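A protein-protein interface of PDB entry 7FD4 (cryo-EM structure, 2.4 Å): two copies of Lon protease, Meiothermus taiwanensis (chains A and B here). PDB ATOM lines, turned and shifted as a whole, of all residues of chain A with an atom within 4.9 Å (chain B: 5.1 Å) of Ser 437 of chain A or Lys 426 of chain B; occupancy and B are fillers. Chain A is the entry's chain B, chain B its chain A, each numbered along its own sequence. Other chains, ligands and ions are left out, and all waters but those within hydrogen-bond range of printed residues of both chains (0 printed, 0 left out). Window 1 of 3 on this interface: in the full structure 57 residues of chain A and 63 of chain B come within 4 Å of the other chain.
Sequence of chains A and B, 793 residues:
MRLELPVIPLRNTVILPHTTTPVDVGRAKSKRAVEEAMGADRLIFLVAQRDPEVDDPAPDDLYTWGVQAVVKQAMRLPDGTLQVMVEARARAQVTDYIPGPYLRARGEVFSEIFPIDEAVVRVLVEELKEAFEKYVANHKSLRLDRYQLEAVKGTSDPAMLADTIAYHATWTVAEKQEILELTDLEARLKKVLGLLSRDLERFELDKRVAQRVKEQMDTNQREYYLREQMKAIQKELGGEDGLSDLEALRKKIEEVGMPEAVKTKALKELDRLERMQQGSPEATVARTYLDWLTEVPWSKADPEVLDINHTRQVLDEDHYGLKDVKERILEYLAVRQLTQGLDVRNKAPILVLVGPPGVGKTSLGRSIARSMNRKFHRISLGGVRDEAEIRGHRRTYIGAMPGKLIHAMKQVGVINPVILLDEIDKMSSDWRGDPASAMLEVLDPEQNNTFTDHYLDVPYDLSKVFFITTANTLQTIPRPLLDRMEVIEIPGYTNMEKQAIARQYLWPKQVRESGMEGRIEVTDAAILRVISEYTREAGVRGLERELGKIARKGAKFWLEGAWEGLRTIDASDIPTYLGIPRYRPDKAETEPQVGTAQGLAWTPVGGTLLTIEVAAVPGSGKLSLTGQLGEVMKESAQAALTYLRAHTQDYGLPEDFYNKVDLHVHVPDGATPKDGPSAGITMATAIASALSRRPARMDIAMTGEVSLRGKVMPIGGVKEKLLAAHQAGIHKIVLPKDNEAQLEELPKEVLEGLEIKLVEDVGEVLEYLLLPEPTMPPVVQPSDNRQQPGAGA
The side-chain hydroxyl (OG) of Ser 437 of chain A is in hydrogen-bond range of the side-chain carboxylate (OD2) of Asp 434 of chain A, 2.7 Å away. OE1 of Glu 423 of chain B is in salt-bridge range of NZ of Lys 426 of chain B. N of Asn 472 of chain B lies within hydrogen-bond range of OD2 of Asp 425 of chain B (3.0 Å).
Among the printed residues, merely in contact across the chains: Asp 434 of chain A with Ser 428 of chain B, Ser 437 of chain A with Gly 382 of chain B, Ser 437 of chain A with Lys 426 of chain B, Leu 440 of chain A with Lys 426 of chain B and Pro 480 of chain A with Asn 472 of chain B.
Printed residues of chain B within 4 Å of Ser 437 of chain A: Gly 382 (3.3 Å) and Lys 426 (3.8 Å). Printed residues of chain B within 4 Å of Asp 434 of chain A: Ser 428. Of the printed residues of chain B, Leu 440 of chain A touches Lys 426. Leu 381 of chain B touches none of the printed residues of chain A. Gly 383 of chain B touches none of the printed residues of chain A. The nearest residue of chain B that does not touch Ser 437 of chain A is Gly 383 of chain B (4.2 Å). The nearest residue of chain A that does not touch Lys 426 of chain B is Pro 480 of chain A (4.5 Å).
Of the 10 printed residues of chain B, 4 touch a printed residue of chain A. Of the 9 printed residues of chain A, 4 touch a printed residue of chain B. Hydrophobic or aromatic side chains of chain A that line the printed part of chain B: Leu 440 and Pro 480. Among the printed residues, no Asp or Glu carboxylate lies within 4 Å of a Lys or Arg side-chain nitrogen of the other chain.
No position is printed for both chains. Of the 5 pairs that touch across the chains among the printed residues, none has its exchanged pair printed and touching as well.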
ATOM      1  N   ASP A 434      21.144  15.908  28.838  1.00  0.00           N
ATOM      2  CA  ASP A 434      22.565  15.664  28.598  1.00  0.00           C
ATOM      3  C   ASP A 434      23.035  16.546  27.457  1.00  0.00           C
ATOM      4  O   ASP A 434      23.117  16.110  26.305  1.00  0.00           O
ATOM      5  CB  ASP A 434      22.815  14.193  28.279  1.00  0.00           C
ATOM      6  CG  ASP A 434      24.269  13.815  28.371  1.00  0.00           C
ATOM      7  OD1 ASP A 434      25.097  14.678  28.714  1.00  0.00           O
ATOM      8  OD2 ASP A 434      24.594  12.643  28.093  1.00  0.00           O
ATOM      9  N   PRO A 435      23.364  17.807  27.739  1.00  0.00           N
ATOM     10  CA  PRO A 435      23.927  18.660  26.692  1.00  0.00           C
ATOM     11  C   PRO A 435      25.426  18.511  26.545  1.00  0.00           C
ATOM     12  O   PRO A 435      25.978  18.977  25.545  1.00  0.00           O
ATOM     13  CB  PRO A 435      23.568  20.060  27.171  1.00  0.00           C
ATOM     14  CG  PRO A 435      23.616  19.939  28.612  1.00  0.00           C
ATOM     15  CD  PRO A 435      23.117  18.577  28.966  1.00  0.00           C
ATOM     16  N   ALA A 436      26.094  17.878  27.507  1.00  0.00           N
ATOM     17  CA  ALA A 436      27.528  17.656  27.420  1.00  0.00           C
ATOM     18  C   ALA A 436      27.889  16.615  26.381  1.00  0.00           C
ATOM     19  O   ALA A 436      29.050  16.529  25.987  1.00  0.00           O
ATOM     20  CB  ALA A 436      28.070  17.225  28.776  1.00  0.00           C
ATOM     21  N   SER A 437      26.927  15.813  25.945  1.00  0.00           N
ATOM     22  CA  SER A 437      27.153  14.838  24.896  1.00  0.00           C
ATOM     23  C   SER A 437      26.915  15.400  23.513  1.00  0.00           C
ATOM     24  O   SER A 437      27.396  14.822  22.539  1.00  0.00           O
ATOM     25  CB  SER A 437      26.253  13.628  25.109  1.00  0.00           C
ATOM     26  OG  SER A 437      26.581  12.977  26.318  1.00  0.00           O
ATOM     27  N   ALA A 438      26.187  16.504  23.400  1.00  0.00           N
ATOM     28  CA  ALA A 438      26.078  17.197  22.131  1.00  0.00           C
ATOM     29  C   ALA A 438      27.229  18.158  21.906  1.00  0.00           C
ATOM     30  O   ALA A 438      27.487  18.538  20.765  1.00  0.00           O
ATOM     31  CB  ALA A 438      24.756  17.948  22.056  1.00  0.00           C
ATOM     32  N   MET A 439      27.931  18.553  22.966  1.00  0.00           N
ATOM     33  CA  MET A 439      29.116  19.384  22.831  1.00  0.00           C
ATOM     34  C   MET A 439      30.317  18.617  22.316  1.00  0.00           C
ATOM     35  O   MET A 439      31.332  19.240  22.014  1.00  0.00           O
ATOM     36  CB  MET A 439      29.474  20.018  24.169  1.00  0.00           C
ATOM     37  CG  MET A 439      28.502  21.050  24.645  1.00  0.00           C
ATOM     38  SD  MET A 439      28.509  22.505  23.611  1.00  0.00           S
ATOM     39  CE  MET A 439      30.059  23.204  24.112  1.00  0.00           C
ATOM     40  N   LEU A 440      30.239  17.293  22.223  1.00  0.00           N
ATOM     41  CA  LEU A 440      31.338  16.532  21.655  1.00  0.00           C
ATOM     42  C   LEU A 440      31.477  16.781  20.169  1.00  0.00           C
ATOM     43  O   LEU A 440      32.567  16.633  19.621  1.00  0.00           O
ATOM     44  CB  LEU A 440      31.146  15.041  21.898  1.00  0.00           C
ATOM     45  CG  LEU A 440      31.212  14.509  23.317  1.00  0.00           C
ATOM     46  CD1 LEU A 440      30.892  13.045  23.317  1.00  0.00           C
ATOM     47  CD2 LEU A 440      32.559  14.745  23.898  1.00  0.00           C
ATOM     48  N   GLU A 441      30.399  17.167  19.504  1.00  0.00           N
ATOM     49  CA  GLU A 441      30.458  17.406  18.075  1.00  0.00           C
ATOM     50  C   GLU A 441      30.936  18.815  17.745  1.00  0.00           C
ATOM     51  O   GLU A 441      31.474  19.036  16.658  1.00  0.00           O
ATOM     52  CB  GLU A 441      29.080  17.147  17.466  1.00  0.00           C
ATOM     53  CG  GLU A 441      29.035  17.097  15.951  1.00  0.00           C
ATOM     54  CD  GLU A 441      27.644  16.876  15.418  1.00  0.00           C
ATOM     55  OE1 GLU A 441      26.706  16.815  16.234  1.00  0.00           O
ATOM     56  OE2 GLU A 441      27.489  16.764  14.187  1.00  0.00           O
ATOM     57  N   PRO A 480      35.794  12.166  27.609  1.00  0.00           N
ATOM     58  CA  PRO A 480      35.905  12.489  26.181  1.00  0.00           C
ATOM     59  C   PRO A 480      35.909  13.969  25.901  1.00  0.00           C
ATOM     60  O   PRO A 480      36.747  14.416  25.124  1.00  0.00           O
ATOM     61  CB  PRO A 480      34.681  11.808  25.571  1.00  0.00           C
ATOM     62  CG  PRO A 480      34.417  10.732  26.422  1.00  0.00           C
ATOM     63  CD  PRO A 480      34.711  11.183  27.795  1.00  0.00           C
ATOM     64  N   LEU B 381      25.049  10.696  16.928  1.00  0.00           N
ATOM     65  CA  LEU B 381      23.945  10.379  17.824  1.00  0.00           C
ATOM     66  C   LEU B 381      24.285  10.778  19.250  1.00  0.00           C
ATOM     67  O   LEU B 381      24.043  10.028  20.191  1.00  0.00           O
ATOM     68  CB  LEU B 381      23.618   8.894  17.768  1.00  0.00           C
ATOM     69  CG  LEU B 381      23.135   8.297  16.456  1.00  0.00           C
ATOM     70  CD1 LEU B 381      23.036   6.812  16.626  1.00  0.00           C
ATOM     71  CD2 LEU B 381      21.805   8.875  16.045  1.00  0.00           C
ATOM     72  N   GLY B 382      24.857  11.969  19.414  1.00  0.00           N
ATOM     73  CA  GLY B 382      25.468  12.328  20.682  1.00  0.00           C
ATOM     74  C   GLY B 382      24.462  12.557  21.791  1.00  0.00           C
ATOM     75  O   GLY B 382      24.538  11.932  22.843  1.00  0.00           O
ATOM     76  N   GLY B 383      23.510  13.445  21.578  1.00  0.00           N
ATOM     77  CA  GLY B 383      22.538  13.680  22.623  1.00  0.00           C
ATOM     78  C   GLY B 383      21.128  13.597  22.100  1.00  0.00           C
ATOM     79  O   GLY B 383      20.232  14.266  22.615  1.00  0.00           O
ATOM     80  N   GLU B 423      28.200   8.096  18.203  1.00  0.00           N
ATOM     81  CA  GLU B 423      28.188   7.909  19.653  1.00  0.00           C
ATOM     82  C   GLU B 423      26.935   7.136  20.027  1.00  0.00           C
ATOM     83  O   GLU B 423      25.911   7.737  20.352  1.00  0.00           O
ATOM     84  CB  GLU B 423      28.232   9.242  20.380  1.00  0.00           C
ATOM     85  CG  GLU B 423      29.484  10.053  20.160  1.00  0.00           C
ATOM     86  CD  GLU B 423      30.710   9.424  20.778  1.00  0.00           C
ATOM     87  OE1 GLU B 423      30.580   8.704  21.789  1.00  0.00           O
ATOM     88  OE2 GLU B 423      31.818   9.672  20.265  1.00  0.00           O
ATOM     89  N   ILE B 424      27.001   5.809  20.000  1.00  0.00           N
ATOM     90  CA  ILE B 424      25.792   5.021  20.194  1.00  0.00           C
ATOM     91  C   ILE B 424      25.558   4.688  21.662  1.00  0.00           C
ATOM     92  O   ILE B 424      24.434   4.319  22.033  1.00  0.00           O
ATOM     93  CB  ILE B 424      25.823   3.749  19.316  1.00  0.00           C
ATOM     94  CG1 ILE B 424      24.408   3.229  19.059  1.00  0.00           C
ATOM     95  CG2 ILE B 424      26.668   2.680  19.948  1.00  0.00           C
ATOM     96  CD1 ILE B 424      24.309   2.241  17.965  1.00  0.00           C
ATOM     97  N   ASP B 425      26.548   4.875  22.522  1.00  0.00           N
ATOM     98  CA  ASP B 425      26.335   4.705  23.947  1.00  0.00           C
ATOM     99  C   ASP B 425      25.827   5.964  24.625  1.00  0.00           C
ATOM    100  O   ASP B 425      25.744   5.997  25.853  1.00  0.00           O
ATOM    101  CB  ASP B 425      27.620   4.240  24.624  1.00  0.00           C
ATOM    102  CG  ASP B 425      28.785   5.165  24.372  1.00  0.00           C
ATOM    103  OD1 ASP B 425      28.671   6.060  23.516  1.00  0.00           O
ATOM    104  OD2 ASP B 425      29.818   5.014  25.052  1.00  0.00           O
ATOM    105  N   LYS B 426      25.491   6.996  23.865  1.00  0.00           N
ATOM    106  CA  LYS B 426      25.180   8.294  24.430  1.00  0.00           C
ATOM    107  C   LYS B 426      23.778   8.782  24.131  1.00  0.00           C
ATOM    108  O   LYS B 426      23.464   9.917  24.487  1.00  0.00           O
ATOM    109  CB  LYS B 426      26.171   9.338  23.920  1.00  0.00           C
ATOM    110  CG  LYS B 426      27.587   9.102  24.314  1.00  0.00           C
ATOM    111  CD  LYS B 426      27.811   9.417  25.755  1.00  0.00           C
ATOM    112  CE  LYS B 426      29.241   9.124  26.099  1.00  0.00           C
ATOM    113  NZ  LYS B 426      30.143   9.983  25.302  1.00  0.00           N
ATOM    114  N   MET B 427      22.934   7.979  23.494  1.00  0.00           N
ATOM    115  CA  MET B 427      21.600   8.439  23.142  1.00  0.00           C
ATOM    116  C   MET B 427      20.741   8.623  24.382  1.00  0.00           C
ATOM    117  O   MET B 427      20.778   7.814  25.310  1.00  0.00           O
ATOM    118  CB  MET B 427      20.920   7.453  22.204  1.00  0.00           C
ATOM    119  CG  MET B 427      21.529   7.360  20.839  1.00  0.00           C
ATOM    120  SD  MET B 427      20.535   6.303  19.787  1.00  0.00           S
ATOM    121  CE  MET B 427      20.901   4.713  20.502  1.00  0.00           C
ATOM    122  N   SER B 428      19.973   9.704  24.395  1.00  0.00           N
ATOM    123  CA  SER B 428      19.083  10.024  25.495  1.00  0.00           C
ATOM    124  C   SER B 428      17.673   9.571  25.165  1.00  0.00           C
ATOM    125  O   SER B 428      17.297   9.456  23.999  1.00  0.00           O
ATOM    126  CB  SER B 428      19.083  11.522  25.788  1.00  0.00           C
ATOM    127  OG  SER B 428      20.354  11.947  26.239  1.00  0.00           O
ATOM    128  N   ASN B 472      32.530   4.291  24.043  1.00  0.00           N
ATOM    129  CA  ASN B 472      33.580   4.309  25.054  1.00  0.00           C
ATOM    130  C   ASN B 472      33.436   3.203  26.083  1.00  0.00           C
ATOM    131  O   ASN B 472      34.437   2.607  26.483  1.00  0.00           O
ATOM    132  CB  ASN B 472      33.602   5.650  25.777  1.00  0.00           C
ATOM    133  CG  ASN B 472      34.177   6.748  24.940  1.00  0.00           C
ATOM    134  OD1 ASN B 472      35.221   6.591  24.326  1.00  0.00           O
ATOM    135  ND2 ASN B 472      33.485   7.868  24.890  1.00  0.00           N
